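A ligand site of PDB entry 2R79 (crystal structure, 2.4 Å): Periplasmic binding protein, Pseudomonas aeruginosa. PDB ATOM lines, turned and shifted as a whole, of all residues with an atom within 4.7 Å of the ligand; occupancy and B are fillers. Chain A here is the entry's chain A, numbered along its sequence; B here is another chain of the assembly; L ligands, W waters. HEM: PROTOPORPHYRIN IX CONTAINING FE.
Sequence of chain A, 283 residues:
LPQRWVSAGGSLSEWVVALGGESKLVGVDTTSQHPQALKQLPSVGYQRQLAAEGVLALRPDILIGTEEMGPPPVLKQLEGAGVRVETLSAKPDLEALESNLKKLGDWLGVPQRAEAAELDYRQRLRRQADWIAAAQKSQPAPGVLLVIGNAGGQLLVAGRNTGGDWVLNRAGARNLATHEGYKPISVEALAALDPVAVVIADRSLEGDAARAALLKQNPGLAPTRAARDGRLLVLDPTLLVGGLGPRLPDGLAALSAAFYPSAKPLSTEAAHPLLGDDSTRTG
The side-chain hydroxyl (OH) of Tyr 46 binds an iron atom (FE) of the ligand.
An oxygen (O2A) of the ligand lies within salt-bridge range of the guanidinium group (NH1) of Arg 203, 3.0 Å away.
NH1 of Arg 48 lies within salt-bridge range of O2D of the ligand (3.7 Å).
NE of Arg 48 lies close to OH of Tyr 46, 2.9 Å away.
OG of Ser 43 of chain B lies within hydrogen-bond range of N of Gly 45 of chain B (3.2 Å).
The backbone carbonyl oxygen (O) of Leu 156 sits at hydrogen-bond distance from the backbone NH (N) of Ile 148 (2.7 Å).
Thr 31 touches the ligand.
Gln 49 touches the ligand (NE2 to CAA, 3.6 Å).
Ile 148 touches the ligand.
Tyr 182 touches the ligand.
CG of Pro 237 touches CBB of the ligand (3.7 Å).
CG2 of Val 241 touches CMC of the ligand, at 3.8 Å.
Ser 43 of chain B touches the ligand.
OE1 of Glu 53 of chain B touches CBD of the ligand, at 3.0 Å.
Gly 54 of chain B touches the ligand.
Hydrophobic or aromatic side chains that line the ligand: Tyr 46, Ile 148, Tyr 182, Pro 237 and Val 241.
12 residues have an atom within 4 Å of the ligand: Thr 31, Tyr 46, Arg 48, Gln 49, Ile 148, Tyr 182, Arg 203, Pro 237, Val 241, Ser 43 of chain B, Glu 53 of chain B and Gly 54 of chain B.
Water W4 lies within hydrogen-bond range of O of Ser 43 of chain B (2.6 Å), O2A of the ligand (2.9 Å) and OD1 of Asn 150 (3.1 Å).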
ATOM      1  N   THR A  30      12.731   8.738  18.079  1.00  0.00           N
ATOM      2  CA  THR A  30      13.343   9.461  19.182  1.00  0.00           C
ATOM      3  C   THR A  30      12.401  10.139  20.192  1.00  0.00           C
ATOM      4  O   THR A  30      12.825  10.440  21.308  1.00  0.00           O
ATOM      5  CB  THR A  30      14.347  10.509  18.656  1.00  0.00           C
ATOM      6  OG1 THR A  30      13.665  11.406  17.778  1.00  0.00           O
ATOM      7  CG2 THR A  30      15.468   9.819  17.891  1.00  0.00           C
ATOM      8  N   THR A  31      11.152  10.402  19.827  1.00  0.00           N
ATOM      9  CA  THR A  31      10.236  11.049  20.781  1.00  0.00           C
ATOM     10  C   THR A  31       9.624  10.053  21.755  1.00  0.00           C
ATOM     11  O   THR A  31       8.929  10.450  22.685  1.00  0.00           O
ATOM     12  CB  THR A  31       9.075  11.799  20.081  1.00  0.00           C
ATOM     13  OG1 THR A  31       8.266  10.873  19.354  1.00  0.00           O
ATOM     14  CG2 THR A  31       9.599  12.883  19.152  1.00  0.00           C
ATOM     15  N   GLN A  33      10.178   8.134  24.663  1.00  0.00           N
ATOM     16  CA  GLN A  33      11.072   8.017  25.798  1.00  0.00           C
ATOM     17  C   GLN A  33      10.404   7.514  27.063  1.00  0.00           C
ATOM     18  O   GLN A  33      10.998   7.534  28.141  1.00  0.00           O
ATOM     19  CB  GLN A  33      11.706   9.384  26.060  1.00  0.00           C
ATOM     20  CG  GLN A  33      12.593   9.884  24.920  1.00  0.00           C
ATOM     21  CD  GLN A  33      12.856  11.369  24.996  1.00  0.00           C
ATOM     22  OE1 GLN A  33      12.996  11.941  26.089  1.00  0.00           O
ATOM     23  NE2 GLN A  33      12.935  12.019  23.845  1.00  0.00           N
ATOM     24  N   TYR A  46      13.907  10.458  14.103  1.00  0.00           N
ATOM     25  CA  TYR A  46      12.820  11.343  14.491  1.00  0.00           C
ATOM     26  C   TYR A  46      11.582  10.986  13.655  1.00  0.00           C
ATOM     27  O   TYR A  46      11.696  10.610  12.486  1.00  0.00           O
ATOM     28  CB  TYR A  46      13.214  12.805  14.252  1.00  0.00           C
ATOM     29  CG  TYR A  46      12.166  13.804  14.669  1.00  0.00           C
ATOM     30  CD1 TYR A  46      11.563  13.732  15.930  1.00  0.00           C
ATOM     31  CD2 TYR A  46      11.796  14.846  13.822  1.00  0.00           C
ATOM     32  CE1 TYR A  46      10.614  14.666  16.324  1.00  0.00           C
ATOM     33  CE2 TYR A  46      10.844  15.784  14.203  1.00  0.00           C
ATOM     34  CZ  TYR A  46      10.254  15.691  15.461  1.00  0.00           C
ATOM     35  OH  TYR A  46       9.303  16.616  15.838  1.00  0.00           O
ATOM     36  N   ARG A  48       9.252  12.801  12.259  1.00  0.00           N
ATOM     37  CA  ARG A  48       9.031  13.606  11.064  1.00  0.00           C
ATOM     38  C   ARG A  48      10.080  13.337   9.979  1.00  0.00           C
ATOM     39  O   ARG A  48       9.926  13.774   8.833  1.00  0.00           O
ATOM     40  CB  ARG A  48       9.038  15.092  11.424  1.00  0.00           C
ATOM     41  CG  ARG A  48       7.931  15.512  12.375  1.00  0.00           C
ATOM     42  CD  ARG A  48       8.074  16.976  12.787  1.00  0.00           C
ATOM     43  NE  ARG A  48       7.240  17.326  13.934  1.00  0.00           N
ATOM     44  CZ  ARG A  48       5.939  17.616  13.874  1.00  0.00           C
ATOM     45  NH1 ARG A  48       5.305  17.611  12.704  1.00  0.00           N
ATOM     46  NH2 ARG A  48       5.279  17.921  14.979  1.00  0.00           N
ATOM     47  N   GLN A  49      11.124  12.604  10.337  1.00  0.00           N
ATOM     48  CA  GLN A  49      12.197  12.283   9.397  1.00  0.00           C
ATOM     49  C   GLN A  49      12.666  10.838   9.536  1.00  0.00           C
ATOM     50  O   GLN A  49      13.844  10.572   9.787  1.00  0.00           O
ATOM     51  CB  GLN A  49      13.373  13.249   9.629  1.00  0.00           C
ATOM     52  CG  GLN A  49      13.049  14.697   9.272  1.00  0.00           C
ATOM     53  CD  GLN A  49      14.027  15.674   9.900  1.00  0.00           C
ATOM     54  OE1 GLN A  49      15.236  15.493   9.827  1.00  0.00           O
ATOM     55  NE2 GLN A  49      13.492  16.721  10.520  1.00  0.00           N
ATOM     56  N   ILE A 148       6.623  26.236  22.779  1.00  0.00           N
ATOM     57  CA  ILE A 148       7.519  25.143  22.456  1.00  0.00           C
ATOM     58  C   ILE A 148       8.845  25.768  22.091  1.00  0.00           C
ATOM     59  O   ILE A 148       8.909  26.628  21.208  1.00  0.00           O
ATOM     60  CB  ILE A 148       7.030  24.315  21.258  1.00  0.00           C
ATOM     61  CG1 ILE A 148       5.617  23.789  21.517  1.00  0.00           C
ATOM     62  CG2 ILE A 148       7.987  23.150  21.042  1.00  0.00           C
ATOM     63  CD1 ILE A 148       5.473  22.980  22.797  1.00  0.00           C
ATOM     64  N   ASN A 150      13.355  25.465  21.517  1.00  0.00           N
ATOM     65  CA  ASN A 150      14.489  24.694  21.035  1.00  0.00           C
ATOM     66  C   ASN A 150      15.697  25.352  21.683  1.00  0.00           C
ATOM     67  O   ASN A 150      16.273  26.291  21.143  1.00  0.00           O
ATOM     68  CB  ASN A 150      14.607  24.797  19.509  1.00  0.00           C
ATOM     69  CG  ASN A 150      15.613  23.815  18.931  1.00  0.00           C
ATOM     70  OD1 ASN A 150      15.924  23.859  17.738  1.00  0.00           O
ATOM     71  ND2 ASN A 150      16.112  22.925  19.770  1.00  0.00           N
ATOM     72  N   GLN A 154      13.643  29.805  18.773  1.00  0.00           N
ATOM     73  CA  GLN A 154      12.661  29.351  17.790  1.00  0.00           C
ATOM     74  C   GLN A 154      11.309  29.053  18.413  1.00  0.00           C
ATOM     75  O   GLN A 154      10.672  28.048  18.108  1.00  0.00           O
ATOM     76  CB  GLN A 154      13.194  28.099  17.092  1.00  0.00           C
ATOM     77  CG  GLN A 154      14.451  28.322  16.281  1.00  0.00           C
ATOM     78  CD  GLN A 154      15.182  27.032  15.960  1.00  0.00           C
ATOM     79  OE1 GLN A 154      14.570  26.014  15.615  1.00  0.00           O
ATOM     80  NE2 GLN A 154      16.513  27.062  16.062  1.00  0.00           N
ATOM     81  N   LEU A 156       7.575  28.600  19.485  1.00  0.00           N
ATOM     82  CA  LEU A 156       6.308  28.360  18.819  1.00  0.00           C
ATOM     83  C   LEU A 156       5.248  28.464  19.919  1.00  0.00           C
ATOM     84  O   LEU A 156       5.353  27.819  20.959  1.00  0.00           O
ATOM     85  CB  LEU A 156       6.268  26.960  18.175  1.00  0.00           C
ATOM     86  CG  LEU A 156       7.051  26.702  16.888  1.00  0.00           C
ATOM     87  CD1 LEU A 156       6.815  25.266  16.439  1.00  0.00           C
ATOM     88  CD2 LEU A 156       6.595  27.672  15.783  1.00  0.00           C
ATOM     89  N   TYR A 182       0.405  25.950  16.000  1.00  0.00           N
ATOM     90  CA  TYR A 182       1.639  26.414  16.627  1.00  0.00           C
ATOM     91  C   TYR A 182       2.254  27.440  15.695  1.00  0.00           C
ATOM     92  O   TYR A 182       2.554  27.137  14.537  1.00  0.00           O
ATOM     93  CB  TYR A 182       2.636  25.263  16.814  1.00  0.00           C
ATOM     94  CG  TYR A 182       2.258  24.290  17.908  1.00  0.00           C
ATOM     95  CD1 TYR A 182       1.612  23.085  17.613  1.00  0.00           C
ATOM     96  CD2 TYR A 182       2.548  24.581  19.244  1.00  0.00           C
ATOM     97  CE1 TYR A 182       1.261  22.186  18.634  1.00  0.00           C
ATOM     98  CE2 TYR A 182       2.195  23.695  20.270  1.00  0.00           C
ATOM     99  CZ  TYR A 182       1.564  22.507  19.954  1.00  0.00           C
ATOM    100  OH  TYR A 182       1.216  21.653  20.976  1.00  0.00           O
ATOM    101  N   ARG A 203      12.665  21.244  23.676  1.00  0.00           N
ATOM    102  CA  ARG A 203      13.163  20.009  23.085  1.00  0.00           C
ATOM    103  C   ARG A 203      14.545  19.598  23.597  1.00  0.00           C
ATOM    104  O   ARG A 203      14.834  18.412  23.708  1.00  0.00           O
ATOM    105  CB  ARG A 203      13.233  20.159  21.564  1.00  0.00           C
ATOM    106  CG  ARG A 203      11.884  20.283  20.875  1.00  0.00           C
ATOM    107  CD  ARG A 203      12.052  20.895  19.499  1.00  0.00           C
ATOM    108  NE  ARG A 203      13.233  20.364  18.805  1.00  0.00           N
ATOM    109  CZ  ARG A 203      13.671  20.798  17.633  1.00  0.00           C
ATOM    110  NH1 ARG A 203      13.041  21.770  16.991  1.00  0.00           N
ATOM    111  NH2 ARG A 203      14.758  20.257  17.088  1.00  0.00           N
ATOM    112  N   PRO A 237       8.333  17.920  27.123  1.00  0.00           N
ATOM    113  CA  PRO A 237       7.877  18.040  25.739  1.00  0.00           C
ATOM    114  C   PRO A 237       7.236  16.802  25.102  1.00  0.00           C
ATOM    115  O   PRO A 237       6.359  16.940  24.245  1.00  0.00           O
ATOM    116  CB  PRO A 237       9.144  18.475  24.992  1.00  0.00           C
ATOM    117  CG  PRO A 237      10.245  17.839  25.800  1.00  0.00           C
ATOM    118  CD  PRO A 237       9.786  18.095  27.231  1.00  0.00           C
ATOM    119  N   THR A 238       7.649  15.605  25.540  1.00  0.00           N
ATOM    120  CA  THR A 238       7.094  14.368  24.983  1.00  0.00           C
ATOM    121  C   THR A 238       5.594  14.244  25.279  1.00  0.00           C
ATOM    122  O   THR A 238       4.877  13.480  24.632  1.00  0.00           O
ATOM    123  CB  THR A 238       7.849  13.107  25.494  1.00  0.00           C
ATOM    124  OG1 THR A 238       7.817  13.074  26.932  1.00  0.00           O
ATOM    125  CG2 THR A 238       9.292  13.142  25.035  1.00  0.00           C
ATOM    126  N   LEU A 240       3.486  16.238  24.521  1.00  0.00           N
ATOM    127  CA  LEU A 240       2.780  16.885  23.409  1.00  0.00           C
ATOM    128  C   LEU A 240       2.988  16.250  22.020  1.00  0.00           C
ATOM    129  O   LEU A 240       2.543  16.793  21.010  1.00  0.00           O
ATOM    130  CB  LEU A 240       3.185  18.365  23.350  1.00  0.00           C
ATOM    131  CG  LEU A 240       3.021  19.154  24.659  1.00  0.00           C
ATOM    132  CD1 LEU A 240       3.590  20.563  24.484  1.00  0.00           C
ATOM    133  CD2 LEU A 240       1.551  19.203  25.047  1.00  0.00           C
ATOM    134  N   VAL A 241       3.670  15.115  21.964  1.00  0.00           N
ATOM    135  CA  VAL A 241       3.921  14.460  20.681  1.00  0.00           C
ATOM    136  C   VAL A 241       3.080  13.195  20.503  1.00  0.00           C
ATOM    137  O   VAL A 241       2.868  12.446  21.460  1.00  0.00           O
ATOM    138  CB  VAL A 241       5.408  14.070  20.547  1.00  0.00           C
ATOM    139  CG1 VAL A 241       5.664  13.510  19.150  1.00  0.00           C
ATOM    140  CG2 VAL A 241       6.293  15.285  20.812  1.00  0.00           C
ATOM    141  N   SER B  43      19.577  20.781  18.024  1.00  0.00           N
ATOM    142  CA  SER B  43      19.980  19.591  17.286  1.00  0.00           C
ATOM    143  C   SER B  43      19.602  19.631  15.810  1.00  0.00           C
ATOM    144  O   SER B  43      18.489  20.023  15.458  1.00  0.00           O
ATOM    145  CB  SER B  43      19.366  18.349  17.922  1.00  0.00           C
ATOM    146  OG  SER B  43      19.593  17.204  17.103  1.00  0.00           O
ATOM    147  N   GLY B  45      19.858  16.861  13.969  1.00  0.00           N
ATOM    148  CA  GLY B  45      19.605  15.458  13.628  1.00  0.00           C
ATOM    149  C   GLY B  45      20.869  14.617  13.513  1.00  0.00           C
ATOM    150  O   GLY B  45      21.950  15.039  13.886  1.00  0.00           O
ATOM    151  N   ALA B  51      18.927  17.501   8.730  1.00  0.00           N
ATOM    152  CA  ALA B  51      17.672  18.207   8.496  1.00  0.00           C
ATOM    153  C   ALA B  51      18.027  19.553   7.882  1.00  0.00           C
ATOM    154  O   ALA B  51      18.517  20.441   8.572  1.00  0.00           O
ATOM    155  CB  ALA B  51      16.926  18.400   9.821  1.00  0.00           C
ATOM    156  N   GLU B  53      16.146  22.136   6.791  1.00  0.00           N
ATOM    157  CA  GLU B  53      15.437  23.199   7.488  1.00  0.00           C
ATOM    158  C   GLU B  53      16.028  23.411   8.886  1.00  0.00           C
ATOM    159  O   GLU B  53      16.010  24.531   9.416  1.00  0.00           O
ATOM    160  CB  GLU B  53      13.946  22.848   7.581  1.00  0.00           C
ATOM    161  CG  GLU B  53      13.116  23.774   8.458  1.00  0.00           C
ATOM    162  CD  GLU B  53      11.650  23.355   8.515  1.00  0.00           C
ATOM    163  OE1 GLU B  53      11.368  22.159   8.757  1.00  0.00           O
ATOM    164  OE2 GLU B  53      10.768  24.229   8.328  1.00  0.00           O
ATOM    165  N   GLY B  54      16.542  22.346   9.484  1.00  0.00           N
ATOM    166  CA  GLY B  54      17.127  22.442  10.805  1.00  0.00           C
ATOM    167  C   GLY B  54      18.388  23.281  10.890  1.00  0.00           C
ATOM    168  O   GLY B  54      18.575  24.046  11.839  1.00  0.00           O
HETATM  169  CHA HEM L   1      11.765  19.662  13.918  1.00  0.00           C
HETATM  170  CHB HEM L   1      13.167  16.792  17.668  1.00  0.00           C
HETATM  171  CHC HEM L   1       9.013  17.808  19.969  1.00  0.00           C
HETATM  172  CHD HEM L   1       7.556  20.579  16.228  1.00  0.00           C
HETATM  173  C1A HEM L   1      12.525  18.776  14.727  1.00  0.00           C
HETATM  174  C2A HEM L   1      13.869  18.287  14.454  1.00  0.00           C
HETATM  175  C3A HEM L   1      14.235  17.474  15.481  1.00  0.00           C
HETATM  176  C4A HEM L   1      13.142  17.479  16.432  1.00  0.00           C
HETATM  177  CMA HEM L   1      15.520  16.650  15.613  1.00  0.00           C
HETATM  178  CAA HEM L   1      14.773  18.606  13.254  1.00  0.00           C
HETATM  179  CBA HEM L   1      15.614  19.872  13.432  1.00  0.00           C
HETATM  180  CGA HEM L   1      14.779  21.141  13.395  1.00  0.00           C
HETATM  181  O1A HEM L   1      14.233  21.472  12.319  1.00  0.00           O
HETATM  182  O2A HEM L   1      14.660  21.815  14.453  1.00  0.00           O
HETATM  183  C1B HEM L   1      12.118  16.750  18.592  1.00  0.00           C
HETATM  184  C2B HEM L   1      12.162  16.056  19.874  1.00  0.00           C
HETATM  185  C3B HEM L   1      10.992  16.349  20.537  1.00  0.00           C
HETATM  186  C4B HEM L   1      10.231  17.207  19.641  1.00  0.00           C
HETATM  187  CMB HEM L   1      13.265  15.101  20.357  1.00  0.00           C
HETATM  188  CAB HEM L   1      10.572  15.884  21.779  1.00  0.00           C
HETATM  189  CBB HEM L   1      11.360  15.820  22.889  1.00  0.00           C
HETATM  190  C1C HEM L   1       8.256  18.650  19.136  1.00  0.00           C
HETATM  191  C2C HEM L   1       7.015  19.277  19.532  1.00  0.00           C
HETATM  192  C3C HEM L   1       6.622  20.094  18.528  1.00  0.00           C
HETATM  193  C4C HEM L   1       7.590  19.889  17.453  1.00  0.00           C
HETATM  194  CMC HEM L   1       6.257  19.058  20.824  1.00  0.00           C
HETATM  195  CAC HEM L   1       5.628  21.077  18.612  1.00  0.00           C
HETATM  196  CBC HEM L   1       4.391  20.941  18.083  1.00  0.00           C
HETATM  197  C1D HEM L   1       8.560  20.534  15.262  1.00  0.00           C
HETATM  198  C2D HEM L   1       8.526  21.326  14.064  1.00  0.00           C
HETATM  199  C3D HEM L   1       9.669  21.052  13.384  1.00  0.00           C
HETATM  200  C4D HEM L   1      10.457  20.133  14.206  1.00  0.00           C
HETATM  201  CMD HEM L   1       7.410  22.269  13.612  1.00  0.00           C
HETATM  202  CAD HEM L   1       9.908  21.563  11.971  1.00  0.00           C
HETATM  203  CBD HEM L   1       9.942  20.517  10.857  1.00  0.00           C
HETATM  204  CGD HEM L   1       8.612  19.808  10.627  1.00  0.00           C
HETATM  205  O1D HEM L   1       8.550  18.957   9.718  1.00  0.00           O
HETATM  206  O2D HEM L   1       7.627  20.105  11.346  1.00  0.00           O
HETATM  207  NA  HEM L   1      12.081  18.240  15.950  1.00  0.00           N
HETATM  208  NB  HEM L   1      10.903  17.419  18.428  1.00  0.00           N
HETATM  209  NC  HEM L   1       8.611  19.021  17.846  1.00  0.00           N
HETATM  210  ND  HEM L   1       9.743  19.791  15.353  1.00  0.00           N
HETATM  211 FE   HEM L   1      10.265  18.475  16.798  1.00  0.00          FE
HETATM  212  O   HOH W   1      17.334  15.538  18.341  1.00  0.00           O
HETATM  213  O   HOH W   2       4.245  17.787  17.432  1.00  0.00           O
HETATM  214  O   HOH W   3      15.599  17.993  19.464  1.00  0.00           O
HETATM  215  O   HOH W   4      17.360  22.372  15.472  1.00  0.00           O
